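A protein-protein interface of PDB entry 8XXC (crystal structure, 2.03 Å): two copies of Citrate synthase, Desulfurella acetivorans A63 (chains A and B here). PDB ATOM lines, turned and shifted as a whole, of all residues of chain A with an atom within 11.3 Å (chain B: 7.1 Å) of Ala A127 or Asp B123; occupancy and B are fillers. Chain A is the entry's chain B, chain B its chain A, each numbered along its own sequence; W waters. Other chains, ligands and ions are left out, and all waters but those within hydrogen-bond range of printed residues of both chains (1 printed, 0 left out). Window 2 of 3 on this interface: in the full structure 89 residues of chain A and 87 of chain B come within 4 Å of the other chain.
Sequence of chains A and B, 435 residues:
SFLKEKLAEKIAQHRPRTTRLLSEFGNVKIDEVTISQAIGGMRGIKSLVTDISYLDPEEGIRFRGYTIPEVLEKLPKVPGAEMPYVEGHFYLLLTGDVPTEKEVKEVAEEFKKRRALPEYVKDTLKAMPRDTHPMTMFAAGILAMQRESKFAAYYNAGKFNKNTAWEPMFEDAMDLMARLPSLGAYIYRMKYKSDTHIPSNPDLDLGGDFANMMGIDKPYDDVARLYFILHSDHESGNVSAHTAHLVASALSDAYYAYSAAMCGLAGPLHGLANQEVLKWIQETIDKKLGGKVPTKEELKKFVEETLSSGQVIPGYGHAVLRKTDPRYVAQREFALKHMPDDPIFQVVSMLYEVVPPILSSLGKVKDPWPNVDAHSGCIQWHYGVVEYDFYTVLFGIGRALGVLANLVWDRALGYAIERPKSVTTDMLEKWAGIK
The side-chain hydroxyl of Thr A132 is in hydrogen-bond range of the backbone carbonyl oxygen of Pro A129. The backbone carbonyl oxygen of Tyr A120 is in hydrogen-bond range of the side-chain hydroxyl of Thr A124 (2.7 Å). OG1 of Thr B124 lies within hydrogen-bond range of O of Tyr B120 (2.7 Å).
Of the 24 printed residues of chain A, 5 touch a printed residue of chain B. Of the 12 printed residues of chain B, 5 touch a printed residue of chain A. Printed residues of chain B that touch a printed residue of chain A: Tyr B120, Asp B123, Thr B124, Ala B127 and Met B128. Among the printed residues, 8 pairs touch across the chains. Among the printed residues, no Asp or Glu carboxylate lies within 4 Å of a Lys or Arg side-chain nitrogen of the other chain.
Of the printed residues of chain B, Asp A123 touches Ala B127 (3.6 Å). Of chain B, only Asp B123, Thr B124 and Ala B127 come within 4 Å of Ala A127. Of the printed residues of chain B, Met A128 touches Thr B124 (3.6 Å). Of the printed residues of chain B, Pro A129 touches Tyr B120 (3.4 Å). Of the printed residues of chain A, Tyr B120 touches Pro A129. No residue of chain A comes within 4 Å of Val B121. No residue of chain A comes within 4 Å of Lys B126. Of chain A, only Asp A123, Thr A124 and Ala A127 come within 4 Å of Ala B127. Of the printed residues of chain A, Met B128 touches Thr A124 (3.6 Å). The nearest printed residue of chain A that does not touch Met B128 is Ala A144 (4.2 Å).
Among the printed residues, merely in contact across the chains: Asp A123 with Ala B127 (3.6 Å), Thr A124 with Ala B127 (3.7 Å), Thr A124 with Met B128 (3.6 Å), Ala A127 with Asp B123 (3.6 Å), Ala A127 with Thr B124 (3.7 Å), Ala A127 with Ala B127 (3.9 Å), Met A128 with Thr B124 (3.6 Å) and Pro A129 with Tyr B120 (3.4 Å).
Water W1 bridges the backbone carbonyl oxygen of Ala A127 (2.6 Å) and the side-chain carboxylate of Asp B123 (2.8 Å).
Asp A123 touches Ala B127, and with the chains exchanged Ala A127 touches Asp B123. Thr A124 touches Ala B127, and with the chains exchanged Ala A127 touches Thr B124. Thr A124 touches Met B128, and with the chains exchanged Met A128 touches Thr B124. Ala B127 touches its own counterpart, Ala A127. Positions printed for both chains: 119, 120, 121, 122, 123, 124, 125, 126, 127, 128 and 186. Of the 8 pairs that touch across the chains among the printed residues, 7 have their exchanged pair printed and touching as well.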
ATOM      1  N   GLU A 119     -24.270  14.088 -33.144  1.00  0.00           N
ATOM      2  CA  GLU A 119     -22.982  14.451 -32.588  1.00  0.00           C
ATOM      3  C   GLU A 119     -23.082  15.858 -31.987  1.00  0.00           C
ATOM      4  O   GLU A 119     -22.485  16.131 -30.940  1.00  0.00           O
ATOM      5  CB  GLU A 119     -21.938  14.314 -33.700  1.00  0.00           C
ATOM      6  CG  GLU A 119     -20.527  14.122 -33.219  1.00  0.00           C
ATOM      7  CD  GLU A 119     -20.261  12.924 -32.311  1.00  0.00           C
ATOM      8  OE1 GLU A 119     -20.888  11.826 -32.490  1.00  0.00           O
ATOM      9  OE2 GLU A 119     -19.417  13.093 -31.425  1.00  0.00           O
ATOM     10  N   TYR A 120     -23.895  16.721 -32.595  1.00  0.00           N
ATOM     11  CA  TYR A 120     -23.999  18.097 -32.109  1.00  0.00           C
ATOM     12  C   TYR A 120     -24.675  18.145 -30.741  1.00  0.00           C
ATOM     13  O   TYR A 120     -24.562  19.161 -30.046  1.00  0.00           O
ATOM     14  CB  TYR A 120     -24.713  19.010 -33.110  1.00  0.00           C
ATOM     15  CG  TYR A 120     -26.189  18.762 -33.341  1.00  0.00           C
ATOM     16  CD1 TYR A 120     -27.141  19.157 -32.412  1.00  0.00           C
ATOM     17  CD2 TYR A 120     -26.646  18.157 -34.510  1.00  0.00           C
ATOM     18  CE1 TYR A 120     -28.499  18.965 -32.635  1.00  0.00           C
ATOM     19  CE2 TYR A 120     -27.995  17.915 -34.732  1.00  0.00           C
ATOM     20  CZ  TYR A 120     -28.923  18.321 -33.787  1.00  0.00           C
ATOM     21  OH  TYR A 120     -30.258  18.090 -33.995  1.00  0.00           O
ATOM     22  N   VAL A 121     -25.389  17.069 -30.361  1.00  0.00           N
ATOM     23  CA  VAL A 121     -25.968  17.045 -29.026  1.00  0.00           C
ATOM     24  C   VAL A 121     -24.840  16.906 -28.010  1.00  0.00           C
ATOM     25  O   VAL A 121     -24.846  17.592 -26.985  1.00  0.00           O
ATOM     26  CB  VAL A 121     -27.036  15.961 -28.846  1.00  0.00           C
ATOM     27  CG1 VAL A 121     -27.467  15.801 -27.397  1.00  0.00           C
ATOM     28  CG2 VAL A 121     -28.234  16.231 -29.724  1.00  0.00           C
ATOM     29  N   LYS A 122     -23.872  16.046 -28.331  1.00  0.00           N
ATOM     30  CA  LYS A 122     -22.693  15.887 -27.499  1.00  0.00           C
ATOM     31  C   LYS A 122     -21.929  17.206 -27.442  1.00  0.00           C
ATOM     32  O   LYS A 122     -21.486  17.599 -26.368  1.00  0.00           O
ATOM     33  CB  LYS A 122     -21.843  14.726 -28.020  1.00  0.00           C
ATOM     34  CG  LYS A 122     -22.582  13.397 -28.046  1.00  0.00           C
ATOM     35  CD  LYS A 122     -21.747  12.228 -28.514  1.00  0.00           C
ATOM     36  CE  LYS A 122     -22.610  10.992 -28.615  1.00  0.00           C
ATOM     37  NZ  LYS A 122     -21.867   9.764 -28.993  1.00  0.00           N
ATOM     38  N   ASP A 123     -21.771  17.879 -28.588  1.00  0.00           N
ATOM     39  CA  ASP A 123     -21.033  19.139 -28.657  1.00  0.00           C
ATOM     40  C   ASP A 123     -21.679  20.177 -27.728  1.00  0.00           C
ATOM     41  O   ASP A 123     -20.985  20.867 -26.991  1.00  0.00           O
ATOM     42  CB  ASP A 123     -20.939  19.709 -30.091  1.00  0.00           C
ATOM     43  CG  ASP A 123     -20.269  18.841 -31.159  1.00  0.00           C
ATOM     44  OD1 ASP A 123     -19.491  17.917 -30.806  1.00  0.00           O
ATOM     45  OD2 ASP A 123     -20.602  19.034 -32.351  1.00  0.00           O
ATOM     46  N   THR A 124     -23.002  20.298 -27.798  1.00  0.00           N
ATOM     47  CA  THR A 124     -23.770  21.232 -26.989  1.00  0.00           C
ATOM     48  C   THR A 124     -23.581  20.938 -25.487  1.00  0.00           C
ATOM     49  O   THR A 124     -23.355  21.840 -24.689  1.00  0.00           O
ATOM     50  CB  THR A 124     -25.238  21.165 -27.444  1.00  0.00           C
ATOM     51  OG1 THR A 124     -25.277  21.509 -28.837  1.00  0.00           O
ATOM     52  CG2 THR A 124     -26.140  22.043 -26.611  1.00  0.00           C
ATOM     53  N   LEU A 125     -23.654  19.665 -25.106  1.00  0.00           N
ATOM     54  CA  LEU A 125     -23.526  19.230 -23.726  1.00  0.00           C
ATOM     55  C   LEU A 125     -22.103  19.439 -23.193  1.00  0.00           C
ATOM     56  O   LEU A 125     -21.924  19.588 -21.981  1.00  0.00           O
ATOM     57  CB  LEU A 125     -23.918  17.749 -23.650  1.00  0.00           C
ATOM     58  CG  LEU A 125     -25.403  17.418 -23.837  1.00  0.00           C
ATOM     59  CD1 LEU A 125     -25.635  15.904 -23.848  1.00  0.00           C
ATOM     60  CD2 LEU A 125     -26.246  18.037 -22.773  1.00  0.00           C
ATOM     61  N   LYS A 126     -21.088  19.419 -24.078  1.00  0.00           N
ATOM     62  CA  LYS A 126     -19.725  19.670 -23.653  1.00  0.00           C
ATOM     63  C   LYS A 126     -19.513  21.167 -23.491  1.00  0.00           C
ATOM     64  O   LYS A 126     -18.651  21.558 -22.723  1.00  0.00           O
ATOM     65  CB  LYS A 126     -18.666  19.175 -24.640  1.00  0.00           C
ATOM     66  CG  LYS A 126     -18.634  17.675 -24.927  1.00  0.00           C
ATOM     67  CD  LYS A 126     -17.598  17.404 -25.971  1.00  0.00           C
ATOM     68  CE  LYS A 126     -17.272  15.950 -26.188  1.00  0.00           C
ATOM     69  NZ  LYS A 126     -16.191  15.863 -27.197  1.00  0.00           N
ATOM     70  N   ALA A 127     -20.252  21.976 -24.259  1.00  0.00           N
ATOM     71  CA  ALA A 127     -20.132  23.428 -24.174  1.00  0.00           C
ATOM     72  C   ALA A 127     -20.821  24.003 -22.925  1.00  0.00           C
ATOM     73  O   ALA A 127     -20.375  25.013 -22.384  1.00  0.00           O
ATOM     74  CB  ALA A 127     -20.693  24.041 -25.418  1.00  0.00           C
ATOM     75  N   MET A 128     -21.942  23.398 -22.510  1.00  0.00           N
ATOM     76  CA  MET A 128     -22.525  23.684 -21.210  1.00  0.00           C
ATOM     77  C   MET A 128     -21.550  23.250 -20.124  1.00  0.00           C
ATOM     78  O   MET A 128     -20.972  22.153 -20.152  1.00  0.00           O
ATOM     79  CB  MET A 128     -23.854  22.977 -20.993  1.00  0.00           C
ATOM     80  CG  MET A 128     -24.956  23.431 -21.977  1.00  0.00           C
ATOM     81  SD  MET A 128     -26.410  22.315 -22.025  1.00  0.00           S
ATOM     82  CE  MET A 128     -27.238  22.869 -20.543  1.00  0.00           C
ATOM     83  N   PRO A 129     -21.390  24.076 -19.078  1.00  0.00           N
ATOM     84  CA  PRO A 129     -20.499  23.704 -17.980  1.00  0.00           C
ATOM     85  C   PRO A 129     -20.795  22.336 -17.364  1.00  0.00           C
ATOM     86  O   PRO A 129     -21.950  21.970 -17.123  1.00  0.00           O
ATOM     87  CB  PRO A 129     -20.671  24.869 -17.007  1.00  0.00           C
ATOM     88  CG  PRO A 129     -21.049  26.037 -17.913  1.00  0.00           C
ATOM     89  CD  PRO A 129     -21.974  25.426 -18.928  1.00  0.00           C
ATOM     90  N   ARG A 130     -19.725  21.576 -17.109  1.00  0.00           N
ATOM     91  CA  ARG A 130     -19.848  20.190 -16.655  1.00  0.00           C
ATOM     92  C   ARG A 130     -20.583  20.163 -15.321  1.00  0.00           C
ATOM     93  O   ARG A 130     -21.213  19.148 -15.029  1.00  0.00           O
ATOM     94  CB  ARG A 130     -18.493  19.498 -16.540  1.00  0.00           C
ATOM     95  CG  ARG A 130     -18.547  17.985 -16.373  1.00  0.00           C
ATOM     96  CD  ARG A 130     -19.222  17.248 -17.501  1.00  0.00           C
ATOM     97  NE  ARG A 130     -18.688  17.679 -18.771  1.00  0.00           N
ATOM     98  CZ  ARG A 130     -17.821  16.988 -19.506  1.00  0.00           C
ATOM     99  NH1 ARG A 130     -17.521  15.741 -19.178  1.00  0.00           N
ATOM    100  NH2 ARG A 130     -17.311  17.525 -20.604  1.00  0.00           N
ATOM    101  N   ASP A 131     -20.594  21.305 -14.584  1.00  0.00           N
ATOM    102  CA  ASP A 131     -21.194  21.353 -13.263  1.00  0.00           C
ATOM    103  C   ASP A 131     -22.692  21.688 -13.345  1.00  0.00           C
ATOM    104  O   ASP A 131     -23.340  21.779 -12.327  1.00  0.00           O
ATOM    105  CB  ASP A 131     -20.449  22.301 -12.316  1.00  0.00           C
ATOM    106  CG  ASP A 131     -20.288  23.716 -12.808  1.00  0.00           C
ATOM    107  OD1 ASP A 131     -20.714  23.997 -13.947  1.00  0.00           O
ATOM    108  OD2 ASP A 131     -19.732  24.548 -12.040  1.00  0.00           O
ATOM    109  N   THR A 132     -23.254  21.782 -14.546  1.00  0.00           N
ATOM    110  CA  THR A 132     -24.686  21.938 -14.744  1.00  0.00           C
ATOM    111  C   THR A 132     -25.469  20.706 -14.277  1.00  0.00           C
ATOM    112  O   THR A 132     -25.077  19.552 -14.516  1.00  0.00           O
ATOM    113  CB  THR A 132     -24.934  22.181 -16.242  1.00  0.00           C
ATOM    114  OG1 THR A 132     -24.126  23.237 -16.750  1.00  0.00           O
ATOM    115  CG2 THR A 132     -26.356  22.542 -16.597  1.00  0.00           C
ATOM    116  N   THR A 136     -30.903  19.889 -16.470  1.00  0.00           N
ATOM    117  CA  THR A 136     -30.673  21.008 -17.375  1.00  0.00           C
ATOM    118  C   THR A 136     -30.039  20.497 -18.680  1.00  0.00           C
ATOM    119  O   THR A 136     -30.409  20.886 -19.782  1.00  0.00           O
ATOM    120  CB  THR A 136     -29.859  22.084 -16.655  1.00  0.00           C
ATOM    121  OG1 THR A 136     -30.606  22.427 -15.483  1.00  0.00           O
ATOM    122  CG2 THR A 136     -29.619  23.281 -17.538  1.00  0.00           C
ATOM    123  N   MET A 137     -29.102  19.574 -18.556  1.00  0.00           N
ATOM    124  CA  MET A 137     -28.436  18.991 -19.706  1.00  0.00           C
ATOM    125  C   MET A 137     -29.421  18.174 -20.530  1.00  0.00           C
ATOM    126  O   MET A 137     -29.357  18.175 -21.772  1.00  0.00           O
ATOM    127  CB  MET A 137     -27.308  18.064 -19.246  1.00  0.00           C
ATOM    128  CG  MET A 137     -26.083  18.796 -18.743  1.00  0.00           C
ATOM    129  SD  MET A 137     -24.672  17.667 -18.509  1.00  0.00           S
ATOM    130  CE  MET A 137     -23.945  17.713 -20.138  1.00  0.00           C
ATOM    131  N   ALA A 140     -31.785  20.415 -22.397  1.00  0.00           N
ATOM    132  CA  ALA A 140     -31.020  21.064 -23.463  1.00  0.00           C
ATOM    133  C   ALA A 140     -30.791  20.130 -24.658  1.00  0.00           C
ATOM    134  O   ALA A 140     -30.827  20.540 -25.828  1.00  0.00           O
ATOM    135  CB  ALA A 140     -29.695  21.465 -22.902  1.00  0.00           C
ATOM    136  N   GLY A 141     -30.463  18.867 -24.340  1.00  0.00           N
ATOM    137  CA  GLY A 141     -30.233  17.844 -25.351  1.00  0.00           C
ATOM    138  C   GLY A 141     -31.462  17.622 -26.214  1.00  0.00           C
ATOM    139  O   GLY A 141     -31.371  17.520 -27.431  1.00  0.00           O
ATOM    140  N   ALA A 144     -32.088  20.861 -28.359  1.00  0.00           N
ATOM    141  CA  ALA A 144     -31.187  21.068 -29.484  1.00  0.00           C
ATOM    142  C   ALA A 144     -31.608  20.228 -30.684  1.00  0.00           C
ATOM    143  O   ALA A 144     -31.427  20.657 -31.829  1.00  0.00           O
ATOM    144  CB  ALA A 144     -29.768  20.773 -29.065  1.00  0.00           C
ATOM    145  N   TYR A 186     -25.499   9.213 -21.883  1.00  0.00           N
ATOM    146  CA  TYR A 186     -24.392  10.096 -22.215  1.00  0.00           C
ATOM    147  C   TYR A 186     -24.168  11.103 -21.086  1.00  0.00           C
ATOM    148  O   TYR A 186     -23.028  11.326 -20.680  1.00  0.00           O
ATOM    149  CB  TYR A 186     -24.592  10.844 -23.540  1.00  0.00           C
ATOM    150  CG  TYR A 186     -23.365  11.608 -23.961  1.00  0.00           C
ATOM    151  CD1 TYR A 186     -22.377  10.958 -24.661  1.00  0.00           C
ATOM    152  CD2 TYR A 186     -23.121  12.925 -23.579  1.00  0.00           C
ATOM    153  CE1 TYR A 186     -21.201  11.590 -25.029  1.00  0.00           C
ATOM    154  CE2 TYR A 186     -21.936  13.575 -23.928  1.00  0.00           C
ATOM    155  CZ  TYR A 186     -20.971  12.901 -24.654  1.00  0.00           C
ATOM    156  OH  TYR A 186     -19.768  13.433 -25.101  1.00  0.00           O
ATOM    157  N   ILE A 187     -25.240  11.735 -20.601  1.00  0.00           N
ATOM    158  CA  ILE A 187     -25.135  12.675 -19.495  1.00  0.00           C
ATOM    159  C   ILE A 187     -24.558  11.934 -18.272  1.00  0.00           C
ATOM    160  O   ILE A 187     -23.667  12.464 -17.610  1.00  0.00           O
ATOM    161  CB  ILE A 187     -26.506  13.352 -19.231  1.00  0.00           C
ATOM    162  CG1 ILE A 187     -26.875  14.420 -20.262  1.00  0.00           C
ATOM    163  CG2 ILE A 187     -26.611  13.930 -17.851  1.00  0.00           C
ATOM    164  CD1 ILE A 187     -28.343  14.764 -20.293  1.00  0.00           C
ATOM    165  N   MET A 190     -20.787  11.228 -18.871  1.00  0.00           N
ATOM    166  CA  MET A 190     -20.000  12.447 -18.995  1.00  0.00           C
ATOM    167  C   MET A 190     -19.828  13.173 -17.669  1.00  0.00           C
ATOM    168  O   MET A 190     -18.825  13.856 -17.470  1.00  0.00           O
ATOM    169  CB  MET A 190     -20.621  13.407 -20.003  1.00  0.00           C
ATOM    170  CG  MET A 190     -21.156  14.683 -19.384  1.00  0.00           C
ATOM    171  SD  MET A 190     -21.939  15.658 -20.619  1.00  0.00           S
ATOM    172  CE  MET A 190     -20.559  16.253 -21.589  1.00  0.00           C
ATOM    173  N   LYS A 191     -20.822  13.084 -16.787  1.00  0.00           N
ATOM    174  CA  LYS A 191     -20.763  13.790 -15.520  1.00  0.00           C
ATOM    175  C   LYS A 191     -20.142  12.886 -14.462  1.00  0.00           C
ATOM    176  O   LYS A 191     -19.349  13.320 -13.640  1.00  0.00           O
ATOM    177  CB  LYS A 191     -22.146  14.280 -15.087  1.00  0.00           C
ATOM    178  CG  LYS A 191     -22.546  15.638 -15.632  1.00  0.00           C
ATOM    179  CD  LYS A 191     -23.851  16.158 -15.016  1.00  0.00           C
ATOM    180  CE  LYS A 191     -23.692  16.709 -13.614  1.00  0.00           C
ATOM    181  NZ  LYS A 191     -23.050  18.047 -13.566  1.00  0.00           N
ATOM    182  N   ASP A 195     -16.347  10.315 -17.907  1.00  0.00           N
ATOM    183  CA  ASP A 195     -16.467  10.730 -19.290  1.00  0.00           C
ATOM    184  C   ASP A 195     -15.851   9.666 -20.193  1.00  0.00           C
ATOM    185  O   ASP A 195     -15.327   9.943 -21.267  1.00  0.00           O
ATOM    186  CB  ASP A 195     -15.915  12.140 -19.489  1.00  0.00           C
ATOM    187  CG  ASP A 195     -16.452  12.855 -20.716  1.00  0.00           C
ATOM    188  OD1 ASP A 195     -17.501  12.408 -21.234  1.00  0.00           O
ATOM    189  OD2 ASP A 195     -15.851  13.882 -21.111  1.00  0.00           O
ATOM    190  N   PRO B 118     -22.980  35.126 -19.508  1.00  0.00           N
ATOM    191  CA  PRO B 118     -21.939  34.125 -19.249  1.00  0.00           C
ATOM    192  C   PRO B 118     -21.363  33.679 -20.582  1.00  0.00           C
ATOM    193  O   PRO B 118     -22.056  33.606 -21.592  1.00  0.00           O
ATOM    194  CB  PRO B 118     -22.664  33.025 -18.487  1.00  0.00           C
ATOM    195  CG  PRO B 118     -23.886  33.700 -17.885  1.00  0.00           C
ATOM    196  CD  PRO B 118     -24.262  34.796 -18.868  1.00  0.00           C
ATOM    197  N   GLU B 119     -20.053  33.501 -20.601  1.00  0.00           N
ATOM    198  CA  GLU B 119     -19.344  33.184 -21.811  1.00  0.00           C
ATOM    199  C   GLU B 119     -19.767  31.787 -22.293  1.00  0.00           C
ATOM    200  O   GLU B 119     -19.917  31.591 -23.500  1.00  0.00           O
ATOM    201  CB  GLU B 119     -17.850  33.308 -21.526  1.00  0.00           C
ATOM    202  CG  GLU B 119     -17.028  33.335 -22.774  1.00  0.00           C
ATOM    203  CD  GLU B 119     -17.237  34.577 -23.629  1.00  0.00           C
ATOM    204  OE1 GLU B 119     -17.470  35.684 -23.083  1.00  0.00           O
ATOM    205  OE2 GLU B 119     -17.158  34.427 -24.820  1.00  0.00           O
ATOM    206  N   TYR B 120     -20.037  30.865 -21.360  1.00  0.00           N
ATOM    207  CA  TYR B 120     -20.518  29.535 -21.732  1.00  0.00           C
ATOM    208  C   TYR B 120     -21.856  29.618 -22.475  1.00  0.00           C
ATOM    209  O   TYR B 120     -22.213  28.672 -23.160  1.00  0.00           O
ATOM    210  CB  TYR B 120     -20.647  28.601 -20.529  1.00  0.00           C
ATOM    211  CG  TYR B 120     -21.725  28.952 -19.518  1.00  0.00           C
ATOM    212  CD1 TYR B 120     -23.080  28.739 -19.768  1.00  0.00           C
ATOM    213  CD2 TYR B 120     -21.368  29.494 -18.290  1.00  0.00           C
ATOM    214  CE1 TYR B 120     -24.044  29.034 -18.814  1.00  0.00           C
ATOM    215  CE2 TYR B 120     -22.315  29.820 -17.331  1.00  0.00           C
ATOM    216  CZ  TYR B 120     -23.656  29.596 -17.603  1.00  0.00           C
ATOM    217  OH  TYR B 120     -24.519  29.939 -16.618  1.00  0.00           O
ATOM    218  N   VAL B 121     -22.581  30.751 -22.406  1.00  0.00           N
ATOM    219  CA  VAL B 121     -23.810  30.837 -23.191  1.00  0.00           C
ATOM    220  C   VAL B 121     -23.432  30.916 -24.675  1.00  0.00           C
ATOM    221  O   VAL B 121     -23.966  30.148 -25.480  1.00  0.00           O
ATOM    222  CB  VAL B 121     -24.709  31.996 -22.708  1.00  0.00           C
ATOM    223  CG1 VAL B 121     -25.734  32.457 -23.741  1.00  0.00           C
ATOM    224  CG2 VAL B 121     -25.412  31.622 -21.391  1.00  0.00           C
ATOM    225  N   LYS B 122     -22.456  31.784 -24.994  1.00  0.00           N
ATOM    226  CA  LYS B 122     -21.944  31.920 -26.353  1.00  0.00           C
ATOM    227  C   LYS B 122     -21.338  30.596 -26.840  1.00  0.00           C
ATOM    228  O   LYS B 122     -21.640  30.197 -27.963  1.00  0.00           O
ATOM    229  CB  LYS B 122     -20.902  33.033 -26.427  1.00  0.00           C
ATOM    230  CG  LYS B 122     -21.420  34.405 -26.024  1.00  0.00           C
ATOM    231  CD  LYS B 122     -20.319  35.421 -25.911  1.00  0.00           C
ATOM    232  CE  LYS B 122     -20.857  36.830 -25.779  1.00  0.00           C
ATOM    233  NZ  LYS B 122     -19.819  37.763 -25.290  1.00  0.00           N
ATOM    234  N   ASP B 123     -20.576  29.892 -25.977  1.00  0.00           N
ATOM    235  CA  ASP B 123     -20.009  28.578 -26.308  1.00  0.00           C
ATOM    236  C   ASP B 123     -21.088  27.570 -26.693  1.00  0.00           C
ATOM    237  O   ASP B 123     -20.967  26.841 -27.660  1.00  0.00           O
ATOM    238  CB  ASP B 123     -19.270  27.937 -25.123  1.00  0.00           C
ATOM    239  CG  ASP B 123     -18.073  28.683 -24.557  1.00  0.00           C
ATOM    240  OD1 ASP B 123     -17.515  29.531 -25.300  1.00  0.00           O
ATOM    241  OD2 ASP B 123     -17.707  28.408 -23.341  1.00  0.00           O
ATOM    242  N   THR B 124     -22.128  27.473 -25.860  1.00  0.00           N
ATOM    243  CA  THR B 124     -23.291  26.634 -26.089  1.00  0.00           C
ATOM    244  C   THR B 124     -24.005  26.978 -27.402  1.00  0.00           C
ATOM    245  O   THR B 124     -24.411  26.078 -28.141  1.00  0.00           O
ATOM    246  CB  THR B 124     -24.239  26.773 -24.892  1.00  0.00           C
ATOM    247  OG1 THR B 124     -23.503  26.420 -23.718  1.00  0.00           O
ATOM    248  CG2 THR B 124     -25.497  25.964 -25.060  1.00  0.00           C
ATOM    249  N   LEU B 125     -24.232  28.264 -27.680  1.00  0.00           N
ATOM    250  CA  LEU B 125     -24.913  28.645 -28.918  1.00  0.00           C
ATOM    251  C   LEU B 125     -24.072  28.311 -30.158  1.00  0.00           C
ATOM    252  O   LEU B 125     -24.635  28.128 -31.241  1.00  0.00           O
ATOM    253  CB  LEU B 125     -25.198  30.154 -28.899  1.00  0.00           C
ATOM    254  CG  LEU B 125     -26.290  30.636 -27.939  1.00  0.00           C
ATOM    255  CD1 LEU B 125     -26.302  32.160 -27.791  1.00  0.00           C
ATOM    256  CD2 LEU B 125     -27.647  30.181 -28.386  1.00  0.00           C
ATOM    257  N   LYS B 126     -22.730  28.341 -30.042  1.00  0.00           N
ATOM    258  CA  LYS B 126     -21.865  28.040 -31.169  1.00  0.00           C
ATOM    259  C   LYS B 126     -21.868  26.530 -31.434  1.00  0.00           C
ATOM    260  O   LYS B 126     -21.648  26.100 -32.560  1.00  0.00           O
ATOM    261  CB  LYS B 126     -20.422  28.469 -30.888  1.00  0.00           C
ATOM    262  CG  LYS B 126     -20.136  29.974 -30.918  1.00  0.00           C
ATOM    263  CD  LYS B 126     -18.689  30.236 -30.542  1.00  0.00           C
ATOM    264  CE  LYS B 126     -18.309  31.675 -30.298  1.00  0.00           C
ATOM    265  NZ  LYS B 126     -16.837  31.742 -30.130  1.00  0.00           N
ATOM    266  N   ALA B 127     -22.094  25.725 -30.396  1.00  0.00           N
ATOM    267  CA  ALA B 127     -22.049  24.266 -30.496  1.00  0.00           C
ATOM    268  C   ALA B 127     -23.342  23.774 -31.104  1.00  0.00           C
ATOM    269  O   ALA B 127     -23.380  22.756 -31.766  1.00  0.00           O
ATOM    270  CB  ALA B 127     -21.873  23.665 -29.120  1.00  0.00           C
ATOM    271  N   MET B 128     -24.432  24.458 -30.807  1.00  0.00           N
ATOM    272  CA  MET B 128     -25.670  24.193 -31.520  1.00  0.00           C
ATOM    273  C   MET B 128     -25.442  24.496 -33.003  1.00  0.00           C
ATOM    274  O   MET B 128     -24.922  25.552 -33.326  1.00  0.00           O
ATOM    275  CB  MET B 128     -26.792  25.084 -30.980  1.00  0.00           C
ATOM    276  CG  MET B 128     -27.169  24.752 -29.556  1.00  0.00           C
ATOM    277  SD  MET B 128     -28.452  25.819 -28.837  1.00  0.00           S
ATOM    278  CE  MET B 128     -29.911  25.049 -29.532  1.00  0.00           C
ATOM    279  N   TYR B 186     -27.240  38.748 -29.516  1.00  0.00           N
ATOM    280  CA  TYR B 186     -26.179  37.801 -29.858  1.00  0.00           C
ATOM    281  C   TYR B 186     -26.651  36.839 -30.958  1.00  0.00           C
ATOM    282  O   TYR B 186     -25.961  36.607 -31.962  1.00  0.00           O
ATOM    283  CB  TYR B 186     -25.703  36.987 -28.640  1.00  0.00           C
ATOM    284  CG  TYR B 186     -24.388  36.313 -28.908  1.00  0.00           C
ATOM    285  CD1 TYR B 186     -24.326  35.072 -29.521  1.00  0.00           C
ATOM    286  CD2 TYR B 186     -23.195  36.975 -28.660  1.00  0.00           C
ATOM    287  CE1 TYR B 186     -23.114  34.488 -29.860  1.00  0.00           C
ATOM    288  CE2 TYR B 186     -21.968  36.402 -28.986  1.00  0.00           C
ATOM    289  CZ  TYR B 186     -21.930  35.143 -29.573  1.00  0.00           C
ATOM    290  OH  TYR B 186     -20.693  34.619 -29.909  1.00  0.00           O
HETATM  291  O   HOH W   1     -17.858  25.780 -22.417  1.00  0.00           O
